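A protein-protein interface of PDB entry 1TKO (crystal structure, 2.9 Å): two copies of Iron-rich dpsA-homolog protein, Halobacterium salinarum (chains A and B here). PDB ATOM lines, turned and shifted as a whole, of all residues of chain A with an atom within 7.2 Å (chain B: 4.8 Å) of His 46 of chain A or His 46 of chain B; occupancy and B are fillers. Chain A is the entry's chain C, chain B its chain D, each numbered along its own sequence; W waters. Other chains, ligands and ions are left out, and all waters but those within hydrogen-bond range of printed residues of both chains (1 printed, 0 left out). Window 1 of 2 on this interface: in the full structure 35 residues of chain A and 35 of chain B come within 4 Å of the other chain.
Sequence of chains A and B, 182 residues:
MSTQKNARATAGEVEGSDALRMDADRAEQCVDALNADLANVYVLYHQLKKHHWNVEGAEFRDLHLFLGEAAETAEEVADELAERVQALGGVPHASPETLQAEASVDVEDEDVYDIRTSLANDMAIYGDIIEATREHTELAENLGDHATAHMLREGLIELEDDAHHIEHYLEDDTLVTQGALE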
ATOM      1  N   ASN A  40      -8.518  16.368  21.808  1.00  0.00           N
ATOM      2  CA  ASN A  40      -7.916  16.123  20.499  1.00  0.00           C
ATOM      3  C   ASN A  40      -7.173  17.343  19.976  1.00  0.00           C
ATOM      4  O   ASN A  40      -6.059  17.229  19.453  1.00  0.00           O
ATOM      5  CB  ASN A  40      -8.974  15.709  19.481  1.00  0.00           C
ATOM      6  CG  ASN A  40      -9.468  14.291  19.690  1.00  0.00           C
ATOM      7  OD1 ASN A  40      -8.686  13.341  19.721  1.00  0.00           O
ATOM      8  ND2 ASN A  40     -10.775  14.142  19.828  1.00  0.00           N
ATOM      9  N   VAL A  41      -7.787  18.513  20.119  1.00  0.00           N
ATOM     10  CA  VAL A  41      -7.169  19.746  19.651  1.00  0.00           C
ATOM     11  C   VAL A  41      -5.911  20.068  20.441  1.00  0.00           C
ATOM     12  O   VAL A  41      -4.920  20.546  19.882  1.00  0.00           O
ATOM     13  CB  VAL A  41      -8.142  20.927  19.748  1.00  0.00           C
ATOM     14  CG1 VAL A  41      -7.433  22.214  19.402  1.00  0.00           C
ATOM     15  CG2 VAL A  41      -9.306  20.701  18.807  1.00  0.00           C
ATOM     16  N   TYR A  42      -5.928  19.802  21.739  1.00  0.00           N
ATOM     17  CA  TYR A  42      -4.747  20.093  22.522  1.00  0.00           C
ATOM     18  C   TYR A  42      -3.568  19.161  22.249  1.00  0.00           C
ATOM     19  O   TYR A  42      -2.421  19.543  22.473  1.00  0.00           O
ATOM     20  CB  TYR A  42      -5.084  20.115  24.008  1.00  0.00           C
ATOM     21  CG  TYR A  42      -4.858  21.478  24.616  1.00  0.00           C
ATOM     22  CD1 TYR A  42      -5.743  22.004  25.549  1.00  0.00           C
ATOM     23  CD2 TYR A  42      -3.774  22.263  24.217  1.00  0.00           C
ATOM     24  CE1 TYR A  42      -5.565  23.279  26.067  1.00  0.00           C
ATOM     25  CE2 TYR A  42      -3.583  23.533  24.725  1.00  0.00           C
ATOM     26  CZ  TYR A  42      -4.481  24.035  25.650  1.00  0.00           C
ATOM     27  OH  TYR A  42      -4.280  25.296  26.161  1.00  0.00           O
ATOM     28  N   VAL A  43      -3.820  17.939  21.782  1.00  0.00           N
ATOM     29  CA  VAL A  43      -2.688  17.083  21.482  1.00  0.00           C
ATOM     30  C   VAL A  43      -2.242  17.542  20.109  1.00  0.00           C
ATOM     31  O   VAL A  43      -1.050  17.510  19.797  1.00  0.00           O
ATOM     32  CB  VAL A  43      -3.022  15.557  21.452  1.00  0.00           C
ATOM     33  CG1 VAL A  43      -3.927  15.192  22.613  1.00  0.00           C
ATOM     34  CG2 VAL A  43      -3.605  15.162  20.122  1.00  0.00           C
ATOM     35  N   LEU A  44      -3.197  17.987  19.294  1.00  0.00           N
ATOM     36  CA  LEU A  44      -2.872  18.490  17.956  1.00  0.00           C
ATOM     37  C   LEU A  44      -1.941  19.690  18.129  1.00  0.00           C
ATOM     38  O   LEU A  44      -0.956  19.847  17.395  1.00  0.00           O
ATOM     39  CB  LEU A  44      -4.134  18.935  17.212  1.00  0.00           C
ATOM     40  CG  LEU A  44      -3.863  19.769  15.950  1.00  0.00           C
ATOM     41  CD1 LEU A  44      -3.030  18.976  14.975  1.00  0.00           C
ATOM     42  CD2 LEU A  44      -5.173  20.185  15.314  1.00  0.00           C
ATOM     43  N   TYR A  45      -2.274  20.535  19.105  1.00  0.00           N
ATOM     44  CA  TYR A  45      -1.479  21.714  19.424  1.00  0.00           C
ATOM     45  C   TYR A  45      -0.022  21.322  19.699  1.00  0.00           C
ATOM     46  O   TYR A  45       0.906  21.847  19.084  1.00  0.00           O
ATOM     47  CB  TYR A  45      -2.066  22.401  20.655  1.00  0.00           C
ATOM     48  CG  TYR A  45      -1.133  23.387  21.323  1.00  0.00           C
ATOM     49  CD1 TYR A  45      -0.855  24.628  20.742  1.00  0.00           C
ATOM     50  CD2 TYR A  45      -0.521  23.075  22.539  1.00  0.00           C
ATOM     51  CE1 TYR A  45       0.009  25.536  21.361  1.00  0.00           C
ATOM     52  CE2 TYR A  45       0.344  23.972  23.162  1.00  0.00           C
ATOM     53  CZ  TYR A  45       0.602  25.197  22.569  1.00  0.00           C
ATOM     54  OH  TYR A  45       1.454  26.074  23.190  1.00  0.00           O
ATOM     55  N   HIS A  46       0.169  20.387  20.624  1.00  0.00           N
ATOM     56  CA  HIS A  46       1.500  19.937  20.985  1.00  0.00           C
ATOM     57  C   HIS A  46       2.243  19.253  19.849  1.00  0.00           C
ATOM     58  O   HIS A  46       3.467  19.324  19.780  1.00  0.00           O
ATOM     59  CB  HIS A  46       1.421  19.022  22.195  1.00  0.00           C
ATOM     60  CG  HIS A  46       1.254  19.755  23.490  1.00  0.00           C
ATOM     61  ND1 HIS A  46       2.291  20.429  24.103  1.00  0.00           N
ATOM     62  CD2 HIS A  46       0.170  19.930  24.283  1.00  0.00           C
ATOM     63  CE1 HIS A  46       1.852  20.985  25.217  1.00  0.00           C
ATOM     64  NE2 HIS A  46       0.567  20.697  25.350  1.00  0.00           N
ATOM     65  N   GLN A  47       1.522  18.597  18.949  1.00  0.00           N
ATOM     66  CA  GLN A  47       2.198  17.939  17.846  1.00  0.00           C
ATOM     67  C   GLN A  47       2.652  18.978  16.834  1.00  0.00           C
ATOM     68  O   GLN A  47       3.763  18.892  16.298  1.00  0.00           O
ATOM     69  CB  GLN A  47       1.287  16.925  17.166  1.00  0.00           C
ATOM     70  CG  GLN A  47       2.009  16.089  16.120  1.00  0.00           C
ATOM     71  CD  GLN A  47       1.584  14.632  16.155  1.00  0.00           C
ATOM     72  OE1 GLN A  47       1.692  13.965  17.195  1.00  0.00           O
ATOM     73  NE2 GLN A  47       1.105  14.124  15.020  1.00  0.00           N
ATOM     74  N   LEU A  48       1.792  19.960  16.563  1.00  0.00           N
ATOM     75  CA  LEU A  48       2.130  21.020  15.626  1.00  0.00           C
ATOM     76  C   LEU A  48       3.329  21.776  16.173  1.00  0.00           C
ATOM     77  O   LEU A  48       4.212  22.158  15.414  1.00  0.00           O
ATOM     78  CB  LEU A  48       0.944  21.958  15.436  1.00  0.00           C
ATOM     79  CG  LEU A  48      -0.189  21.396  14.595  1.00  0.00           C
ATOM     80  CD1 LEU A  48      -1.323  22.374  14.562  1.00  0.00           C
ATOM     81  CD2 LEU A  48       0.306  21.118  13.192  1.00  0.00           C
ATOM     82  N   LYS A  49       3.361  22.001  17.486  1.00  0.00           N
ATOM     83  CA  LYS A  49       4.512  22.670  18.094  1.00  0.00           C
ATOM     84  C   LYS A  49       5.769  21.834  17.805  1.00  0.00           C
ATOM     85  O   LYS A  49       6.769  22.339  17.306  1.00  0.00           O
ATOM     86  CB  LYS A  49       4.346  22.777  19.604  1.00  0.00           C
ATOM     87  CG  LYS A  49       3.177  23.609  20.032  1.00  0.00           C
ATOM     88  CD  LYS A  49       3.343  25.063  19.651  1.00  0.00           C
ATOM     89  CE  LYS A  49       4.600  25.637  20.248  1.00  0.00           C
ATOM     90  NZ  LYS A  49       4.527  27.115  20.363  1.00  0.00           N
ATOM     91  N   LYS A  50       5.705  20.549  18.139  1.00  0.00           N
ATOM     92  CA  LYS A  50       6.813  19.644  17.918  1.00  0.00           C
ATOM     93  C   LYS A  50       7.362  19.798  16.506  1.00  0.00           C
ATOM     94  O   LYS A  50       8.554  20.039  16.333  1.00  0.00           O
ATOM     95  CB  LYS A  50       6.357  18.209  18.151  1.00  0.00           C
ATOM     96  CG  LYS A  50       7.382  17.164  17.795  1.00  0.00           C
ATOM     97  CD  LYS A  50       6.837  15.787  18.073  1.00  0.00           C
ATOM     98  CE  LYS A  50       7.785  14.684  17.612  1.00  0.00           C
ATOM     99  NZ  LYS A  50       7.209  13.335  17.870  1.00  0.00           N
ATOM    100  N   HIS A  51       6.507  19.664  15.499  1.00  0.00           N
ATOM    101  CA  HIS A  51       6.952  19.796  14.110  1.00  0.00           C
ATOM    102  C   HIS A  51       7.479  21.191  13.809  1.00  0.00           C
ATOM    103  O   HIS A  51       8.363  21.370  12.976  1.00  0.00           O
ATOM    104  CB  HIS A  51       5.806  19.445  13.176  1.00  0.00           C
ATOM    105  CG  HIS A  51       5.313  18.049  13.364  1.00  0.00           C
ATOM    106  ND1 HIS A  51       4.091  17.615  12.898  1.00  0.00           N
ATOM    107  CD2 HIS A  51       5.878  16.986  13.985  1.00  0.00           C
ATOM    108  CE1 HIS A  51       3.923  16.346  13.225  1.00  0.00           C
ATOM    109  NE2 HIS A  51       4.994  15.941  13.885  1.00  0.00           N
ATOM    110  N   HIS A  52       6.920  22.170  14.509  1.00  0.00           N
ATOM    111  CA  HIS A  52       7.305  23.569  14.379  1.00  0.00           C
ATOM    112  C   HIS A  52       8.767  23.694  14.799  1.00  0.00           C
ATOM    113  O   HIS A  52       9.579  24.284  14.086  1.00  0.00           O
ATOM    114  CB  HIS A  52       6.402  24.410  15.287  1.00  0.00           C
ATOM    115  CG  HIS A  52       6.872  25.812  15.493  1.00  0.00           C
ATOM    116  ND1 HIS A  52       6.834  26.767  14.499  1.00  0.00           N
ATOM    117  CD2 HIS A  52       7.380  26.427  16.586  1.00  0.00           C
ATOM    118  CE1 HIS A  52       7.297  27.908  14.971  1.00  0.00           C
ATOM    119  NE2 HIS A  52       7.638  27.729  16.237  1.00  0.00           N
ATOM    120  N   TRP A  53       9.096  23.116  15.952  1.00  0.00           N
ATOM    121  CA  TRP A  53      10.449  23.164  16.491  1.00  0.00           C
ATOM    122  C   TRP A  53      11.464  22.373  15.675  1.00  0.00           C
ATOM    123  O   TRP A  53      12.586  22.826  15.455  1.00  0.00           O
ATOM    124  CB  TRP A  53      10.497  22.612  17.916  1.00  0.00           C
ATOM    125  CG  TRP A  53       9.620  23.287  18.912  1.00  0.00           C
ATOM    126  CD1 TRP A  53       9.419  24.633  19.062  1.00  0.00           C
ATOM    127  CD2 TRP A  53       8.906  22.658  19.984  1.00  0.00           C
ATOM    128  NE1 TRP A  53       8.633  24.881  20.169  1.00  0.00           N
ATOM    129  CE2 TRP A  53       8.308  23.686  20.752  1.00  0.00           C
ATOM    130  CE3 TRP A  53       8.725  21.325  20.377  1.00  0.00           C
ATOM    131  CZ2 TRP A  53       7.533  23.421  21.883  1.00  0.00           C
ATOM    132  CZ3 TRP A  53       7.953  21.060  21.507  1.00  0.00           C
ATOM    133  CH2 TRP A  53       7.369  22.108  22.249  1.00  0.00           C
ATOM    134  N   ALA A  71      -0.365  25.923  15.107  1.00  0.00           N
ATOM    135  CA  ALA A  71      -0.337  25.630  16.534  1.00  0.00           C
ATOM    136  C   ALA A  71      -1.164  26.675  17.273  1.00  0.00           C
ATOM    137  O   ALA A  71      -1.959  26.337  18.141  1.00  0.00           O
ATOM    138  CB  ALA A  71       1.085  25.643  17.044  1.00  0.00           C
ATOM    139  N   ALA A  74      -4.868  26.195  16.842  1.00  0.00           N
ATOM    140  CA  ALA A  74      -5.315  25.072  17.637  1.00  0.00           C
ATOM    141  C   ALA A  74      -5.496  25.498  19.079  1.00  0.00           C
ATOM    142  O   ALA A  74      -6.485  25.151  19.706  1.00  0.00           O
ATOM    143  CB  ALA A  74      -4.320  23.944  17.548  1.00  0.00           C
ATOM    144  N   HIS A  93     -11.041  19.269  30.527  1.00  0.00           N
ATOM    145  CA  HIS A  93      -9.842  18.502  30.806  1.00  0.00           C
ATOM    146  C   HIS A  93      -8.716  19.523  30.952  1.00  0.00           C
ATOM    147  O   HIS A  93      -8.728  20.545  30.276  1.00  0.00           O
ATOM    148  CB  HIS A  93      -9.554  17.529  29.661  1.00  0.00           C
ATOM    149  CG  HIS A  93     -10.633  16.507  29.441  1.00  0.00           C
ATOM    150  ND1 HIS A  93     -11.211  15.797  30.471  1.00  0.00           N
ATOM    151  CD2 HIS A  93     -11.219  16.057  28.303  1.00  0.00           C
ATOM    152  CE1 HIS A  93     -12.104  14.955  29.979  1.00  0.00           C
ATOM    153  NE2 HIS A  93     -12.128  15.092  28.667  1.00  0.00           N
ATOM    154  N   ALA A  94      -7.746  19.271  31.827  1.00  0.00           N
ATOM    155  CA  ALA A  94      -6.683  20.246  32.030  1.00  0.00           C
ATOM    156  C   ALA A  94      -5.243  19.751  31.994  1.00  0.00           C
ATOM    157  O   ALA A  94      -4.434  20.289  31.244  1.00  0.00           O
ATOM    158  CB  ALA A  94      -6.923  20.998  33.335  1.00  0.00           C
ATOM    159  N   SER A  95      -4.900  18.749  32.797  1.00  0.00           N
ATOM    160  CA  SER A  95      -3.523  18.262  32.812  1.00  0.00           C
ATOM    161  C   SER A  95      -3.104  17.651  31.482  1.00  0.00           C
ATOM    162  O   SER A  95      -3.927  17.090  30.758  1.00  0.00           O
ATOM    163  CB  SER A  95      -3.328  17.225  33.922  1.00  0.00           C
ATOM    164  OG  SER A  95      -3.961  15.997  33.604  1.00  0.00           O
ATOM    165  N   PRO A  96      -1.809  17.764  31.138  1.00  0.00           N
ATOM    166  CA  PRO A  96      -1.302  17.207  29.880  1.00  0.00           C
ATOM    167  C   PRO A  96      -1.618  15.718  29.812  1.00  0.00           C
ATOM    168  O   PRO A  96      -1.982  15.198  28.761  1.00  0.00           O
ATOM    169  CB  PRO A  96       0.198  17.474  29.965  1.00  0.00           C
ATOM    170  CG  PRO A  96       0.274  18.722  30.777  1.00  0.00           C
ATOM    171  CD  PRO A  96      -0.737  18.468  31.868  1.00  0.00           C
ATOM    172  N   GLU A  97      -1.482  15.052  30.955  1.00  0.00           N
ATOM    173  CA  GLU A  97      -1.743  13.620  31.088  1.00  0.00           C
ATOM    174  C   GLU A  97      -3.186  13.297  30.733  1.00  0.00           C
ATOM    175  O   GLU A  97      -3.446  12.404  29.939  1.00  0.00           O
ATOM    176  CB  GLU A  97      -1.463  13.179  32.524  1.00  0.00           C
ATOM    177  CG  GLU A  97      -1.382  11.674  32.721  1.00  0.00           C
ATOM    178  CD  GLU A  97      -1.183  11.296  34.187  1.00  0.00           C
ATOM    179  OE1 GLU A  97      -2.125  11.500  34.991  1.00  0.00           O
ATOM    180  OE2 GLU A  97      -0.082  10.805  34.539  1.00  0.00           O
ATOM    181  N   LEU A  99      -5.314  15.193  29.089  1.00  0.00           N
ATOM    182  CA  LEU A  99      -5.581  15.564  27.707  1.00  0.00           C
ATOM    183  C   LEU A  99      -5.213  14.455  26.728  1.00  0.00           C
ATOM    184  O   LEU A  99      -6.025  14.099  25.876  1.00  0.00           O
ATOM    185  CB  LEU A  99      -4.858  16.873  27.345  1.00  0.00           C
ATOM    186  CG  LEU A  99      -5.385  18.154  28.003  1.00  0.00           C
ATOM    187  CD1 LEU A  99      -4.501  19.317  27.612  1.00  0.00           C
ATOM    188  CD2 LEU A  99      -6.816  18.418  27.574  1.00  0.00           C
ATOM    189  N   GLN A 100      -4.013  13.894  26.845  1.00  0.00           N
ATOM    190  CA  GLN A 100      -3.614  12.829  25.925  1.00  0.00           C
ATOM    191  C   GLN A 100      -4.456  11.575  26.135  1.00  0.00           C
ATOM    192  O   GLN A 100      -4.901  10.947  25.170  1.00  0.00           O
ATOM    193  CB  GLN A 100      -2.134  12.485  26.085  1.00  0.00           C
ATOM    194  CG  GLN A 100      -1.622  11.577  24.985  1.00  0.00           C
ATOM    195  CD  GLN A 100      -0.135  11.727  24.773  1.00  0.00           C
ATOM    196  OE1 GLN A 100       0.486  12.634  25.323  1.00  0.00           O
ATOM    197  NE2 GLN A 100       0.445  10.852  23.963  1.00  0.00           N
ATOM    198  N   TYR B  42       5.671  23.793  30.744  1.00  0.00           N
ATOM    199  CA  TYR B  42       4.487  23.411  30.006  1.00  0.00           C
ATOM    200  C   TYR B  42       3.356  22.866  30.873  1.00  0.00           C
ATOM    201  O   TYR B  42       2.193  22.968  30.487  1.00  0.00           O
ATOM    202  CB  TYR B  42       4.838  22.429  28.903  1.00  0.00           C
ATOM    203  CG  TYR B  42       4.572  23.013  27.550  1.00  0.00           C
ATOM    204  CD1 TYR B  42       5.453  22.805  26.493  1.00  0.00           C
ATOM    205  CD2 TYR B  42       3.441  23.804  27.328  1.00  0.00           C
ATOM    206  CE1 TYR B  42       5.211  23.378  25.238  1.00  0.00           C
ATOM    207  CE2 TYR B  42       3.187  24.377  26.087  1.00  0.00           C
ATOM    208  CZ  TYR B  42       4.071  24.164  25.045  1.00  0.00           C
ATOM    209  OH  TYR B  42       3.816  24.725  23.809  1.00  0.00           O
ATOM    210  N   VAL B  43       3.655  22.278  32.031  1.00  0.00           N
ATOM    211  CA  VAL B  43       2.557  21.810  32.856  1.00  0.00           C
ATOM    212  C   VAL B  43       2.065  23.073  33.559  1.00  0.00           C
ATOM    213  O   VAL B  43       0.877  23.207  33.851  1.00  0.00           O
ATOM    214  CB  VAL B  43       2.977  20.730  33.901  1.00  0.00           C
ATOM    215  CG1 VAL B  43       3.961  19.748  33.286  1.00  0.00           C
ATOM    216  CG2 VAL B  43       3.538  21.373  35.154  1.00  0.00           C
ATOM    217  N   LEU B  44       2.979  24.013  33.811  1.00  0.00           N
ATOM    218  CA  LEU B  44       2.617  25.269  34.456  1.00  0.00           C
ATOM    219  C   LEU B  44       1.625  25.972  33.539  1.00  0.00           C
ATOM    220  O   LEU B  44       0.624  26.548  33.986  1.00  0.00           O
ATOM    221  CB  LEU B  44       3.845  26.161  34.650  1.00  0.00           C
ATOM    222  CG  LEU B  44       3.503  27.619  35.012  1.00  0.00           C
ATOM    223  CD1 LEU B  44       2.696  27.669  36.304  1.00  0.00           C
ATOM    224  CD2 LEU B  44       4.772  28.430  35.151  1.00  0.00           C
ATOM    225  N   TYR B  45       1.919  25.915  32.245  1.00  0.00           N
ATOM    226  CA  TYR B  45       1.071  26.521  31.229  1.00  0.00           C
ATOM    227  C   TYR B  45      -0.344  25.982  31.332  1.00  0.00           C
ATOM    228  O   TYR B  45      -1.309  26.742  31.451  1.00  0.00           O
ATOM    229  CB  TYR B  45       1.634  26.211  29.845  1.00  0.00           C
ATOM    230  CG  TYR B  45       0.668  26.432  28.712  1.00  0.00           C
ATOM    231  CD1 TYR B  45       0.307  27.714  28.309  1.00  0.00           C
ATOM    232  CD2 TYR B  45       0.106  25.353  28.048  1.00  0.00           C
ATOM    233  CE1 TYR B  45      -0.599  27.910  27.266  1.00  0.00           C
ATOM    234  CE2 TYR B  45      -0.798  25.533  27.014  1.00  0.00           C
ATOM    235  CZ  TYR B  45      -1.146  26.811  26.630  1.00  0.00           C
ATOM    236  OH  TYR B  45      -2.050  26.972  25.616  1.00  0.00           O
ATOM    237  N   HIS B  46      -0.463  24.659  31.295  1.00  0.00           N
ATOM    238  CA  HIS B  46      -1.765  24.011  31.374  1.00  0.00           C
ATOM    239  C   HIS B  46      -2.507  24.238  32.695  1.00  0.00           C
ATOM    240  O   HIS B  46      -3.744  24.244  32.722  1.00  0.00           O
ATOM    241  CB  HIS B  46      -1.611  22.521  31.108  1.00  0.00           C
ATOM    242  CG  HIS B  46      -1.462  22.180  29.659  1.00  0.00           C
ATOM    243  ND1 HIS B  46      -2.524  22.193  28.779  1.00  0.00           N
ATOM    244  CD2 HIS B  46      -0.376  21.818  28.934  1.00  0.00           C
ATOM    245  CE1 HIS B  46      -2.097  21.852  27.576  1.00  0.00           C
ATOM    246  NE2 HIS B  46      -0.796  21.619  27.643  1.00  0.00           N
ATOM    247  N   GLN B  47      -1.770  24.423  33.785  1.00  0.00           N
ATOM    248  CA  GLN B  47      -2.414  24.662  35.062  1.00  0.00           C
ATOM    249  C   GLN B  47      -2.943  26.089  35.110  1.00  0.00           C
ATOM    250  O   GLN B  47      -4.046  26.337  35.612  1.00  0.00           O
ATOM    251  CB  GLN B  47      -1.446  24.439  36.210  1.00  0.00           C
ATOM    252  CG  GLN B  47      -2.146  24.498  37.548  1.00  0.00           C
ATOM    253  CD  GLN B  47      -1.653  23.452  38.523  1.00  0.00           C
ATOM    254  OE1 GLN B  47      -1.707  22.248  38.252  1.00  0.00           O
ATOM    255  NE2 GLN B  47      -1.179  23.909  39.673  1.00  0.00           N
ATOM    256  N   LEU B  48      -2.152  27.030  34.593  1.00  0.00           N
ATOM    257  CA  LEU B  48      -2.568  28.424  34.563  1.00  0.00           C
ATOM    258  C   LEU B  48      -3.795  28.531  33.678  1.00  0.00           C
ATOM    259  O   LEU B  48      -4.717  29.267  33.997  1.00  0.00           O
ATOM    260  CB  LEU B  48      -1.448  29.315  34.041  1.00  0.00           C
ATOM    261  CG  LEU B  48      -0.300  29.556  35.019  1.00  0.00           C
ATOM    262  CD1 LEU B  48       0.788  30.370  34.355  1.00  0.00           C
ATOM    263  CD2 LEU B  48      -0.816  30.287  36.227  1.00  0.00           C
ATOM    264  N   LYS B  49      -3.818  27.790  32.574  1.00  0.00           N
ATOM    265  CA  LYS B  49      -4.991  27.811  31.697  1.00  0.00           C
ATOM    266  C   LYS B  49      -6.195  27.349  32.510  1.00  0.00           C
ATOM    267  O   LYS B  49      -7.226  28.014  32.562  1.00  0.00           O
ATOM    268  CB  LYS B  49      -4.814  26.863  30.513  1.00  0.00           C
ATOM    269  CG  LYS B  49      -3.680  27.226  29.597  1.00  0.00           C
ATOM    270  CD  LYS B  49      -3.929  28.549  28.885  1.00  0.00           C
ATOM    271  CE  LYS B  49      -5.213  28.515  28.101  1.00  0.00           C
ATOM    272  NZ  LYS B  49      -5.189  29.519  27.005  1.00  0.00           N
ATOM    273  N   LYS B  50      -6.057  26.188  33.134  1.00  0.00           N
ATOM    274  CA  LYS B  50      -7.114  25.627  33.957  1.00  0.00           C
ATOM    275  C   LYS B  50      -7.704  26.679  34.891  1.00  0.00           C
ATOM    276  O   LYS B  50      -8.904  26.924  34.887  1.00  0.00           O
ATOM    277  CB  LYS B  50      -6.555  24.463  34.772  1.00  0.00           C
ATOM    278  CG  LYS B  50      -7.521  23.855  35.742  1.00  0.00           C
ATOM    279  CD  LYS B  50      -6.904  22.670  36.436  1.00  0.00           C
ATOM    280  CE  LYS B  50      -7.816  22.139  37.517  1.00  0.00           C
ATOM    281  NZ  LYS B  50      -7.164  21.019  38.230  1.00  0.00           N
ATOM    282  N   ALA B  94       7.732  16.596  23.664  1.00  0.00           N
ATOM    283  CA  ALA B  94       6.617  17.123  22.887  1.00  0.00           C
ATOM    284  C   ALA B  94       5.204  16.721  23.298  1.00  0.00           C
ATOM    285  O   ALA B  94       4.365  17.594  23.506  1.00  0.00           O
ATOM    286  CB  ALA B  94       6.830  16.802  21.421  1.00  0.00           C
ATOM    287  N   PRO B  96       1.855  15.674  25.364  1.00  0.00           N
ATOM    288  CA  PRO B  96       1.353  16.089  26.678  1.00  0.00           C
ATOM    289  C   PRO B  96       1.749  15.062  27.739  1.00  0.00           C
ATOM    290  O   PRO B  96       2.120  15.410  28.864  1.00  0.00           O
ATOM    291  CB  PRO B  96      -0.159  16.142  26.466  1.00  0.00           C
ATOM    292  CG  PRO B  96      -0.283  16.501  25.026  1.00  0.00           C
ATOM    293  CD  PRO B  96       0.760  15.626  24.379  1.00  0.00           C
ATOM    294  N   LEU B  99       5.444  15.392  28.550  1.00  0.00           N
ATOM    295  CA  LEU B  99       5.673  16.619  29.290  1.00  0.00           C
ATOM    296  C   LEU B  99       5.344  16.463  30.763  1.00  0.00           C
ATOM    297  O   LEU B  99       6.146  16.844  31.603  1.00  0.00           O
ATOM    298  CB  LEU B  99       4.876  17.787  28.679  1.00  0.00           C
ATOM    299  CG  LEU B  99       5.348  18.305  27.310  1.00  0.00           C
ATOM    300  CD1 LEU B  99       4.397  19.372  26.813  1.00  0.00           C
ATOM    301  CD2 LEU B  99       6.763  18.846  27.408  1.00  0.00           C
HETATM  302  O   HOH W   1       4.614  19.975  22.611  1.00  0.00           O
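Among the printed residues, pairs that only touch across the chains: Tyr 42 of chain A with His 46 of chain B, Tyr 42 of chain A with Lys 49 of chain B, His 46 of chain A with Tyr 42 of chain B, His 46 of chain A with Ala 94 of chain B, His 46 of chain A with Pro 96 of chain B, His 46 of chain A with Leu 99 of chain B, Lys 49 of chain A with Tyr 42 of chain B, Lys 50 of chain A with Ala 94 of chain B, Trp 53 of chain A with Tyr 42 of chain B, Ala 94 of chain A with His 46 of chain B, Ala 94 of chain A with Lys 50 of chain B, Pro 96 of chain A with His 46 of chain B, Pro 96 of chain A with Pro 96 of chain B and Leu 99 of chain A with His 46 of chain B.
Water W1 bridges O of Ala 94 of chain B and ND1 of His 46 of chain A.
OE1 of Gln 100 of chain A lies close to N of Pro 96 of chain B (3.3 Å). The side-chain hydroxyl (OH) of Tyr 42 of chain A lies within hydrogen-bond range of the side-chain hydroxyl (OH) of Tyr 45 of chain B (2.8 Å). A ring nitrogen (NE2) of His 46 of chain A sits at hydrogen-bond distance from a ring nitrogen (NE2) of His 46 of chain B. The side-chain hydroxyl (OH) of Tyr 42 of chain B is in hydrogen-bond range of the side-chain hydroxyl (OH) of Tyr 45 of chain A.
His 46 of chain A touches just these residues of chain B: Tyr 42, His 46, Ala 94, Pro 96 and Leu 99. His 46 of chain B touches just these residues of chain A: Tyr 42 (3.6 Å), His 46 (2.8 Å), Ala 94 (3.6 Å), Pro 96 (3.7 Å) and Leu 99 (3.5 Å). Printed residues of chain A within 4 Å of Ala 94 of chain B: His 46 and Lys 50. Of the printed residues of chain A, Tyr 45 of chain B touches Tyr 42 (2.8 Å). Printed residues of chain B within 4 Å of Leu 99 of chain A: His 46. Of the printed residues of chain B, Tyr 42 of chain A touches Tyr 45 (2.8 Å), His 46 (3.6 Å) and Lys 49 (3.9 Å). Leu 48 of chain B touches none of the printed residues of chain A. The nearest printed residue of chain B that does not touch His 46 of chain A is Tyr 45 of chain B (5.3 Å).
Tyr 42 of chain A touches His 46 of chain B, and with the chains exchanged His 46 of chain A touches Tyr 42 of chain B. Tyr 42 of chain A touches Lys 49 of chain B, and with the chains exchanged Lys 49 of chain A touches Tyr 42 of chain B. His 46 of chain A touches Ala 94 of chain B, and with the chains exchanged Ala 94 of chain A touches His 46 of chain B. Pro 96 of chain A touches its own counterpart, Pro 96 of chain B.
Printed residues of chain B that touch a printed residue of chain A: Tyr 42, Tyr 45, His 46, Lys 49, Lys 50, Ala 94, Pro 96 and Leu 99. Among the printed residues, no Asp or Glu carboxylate lies within 4 Å of a Lys or Arg side-chain nitrogen of the other chain.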
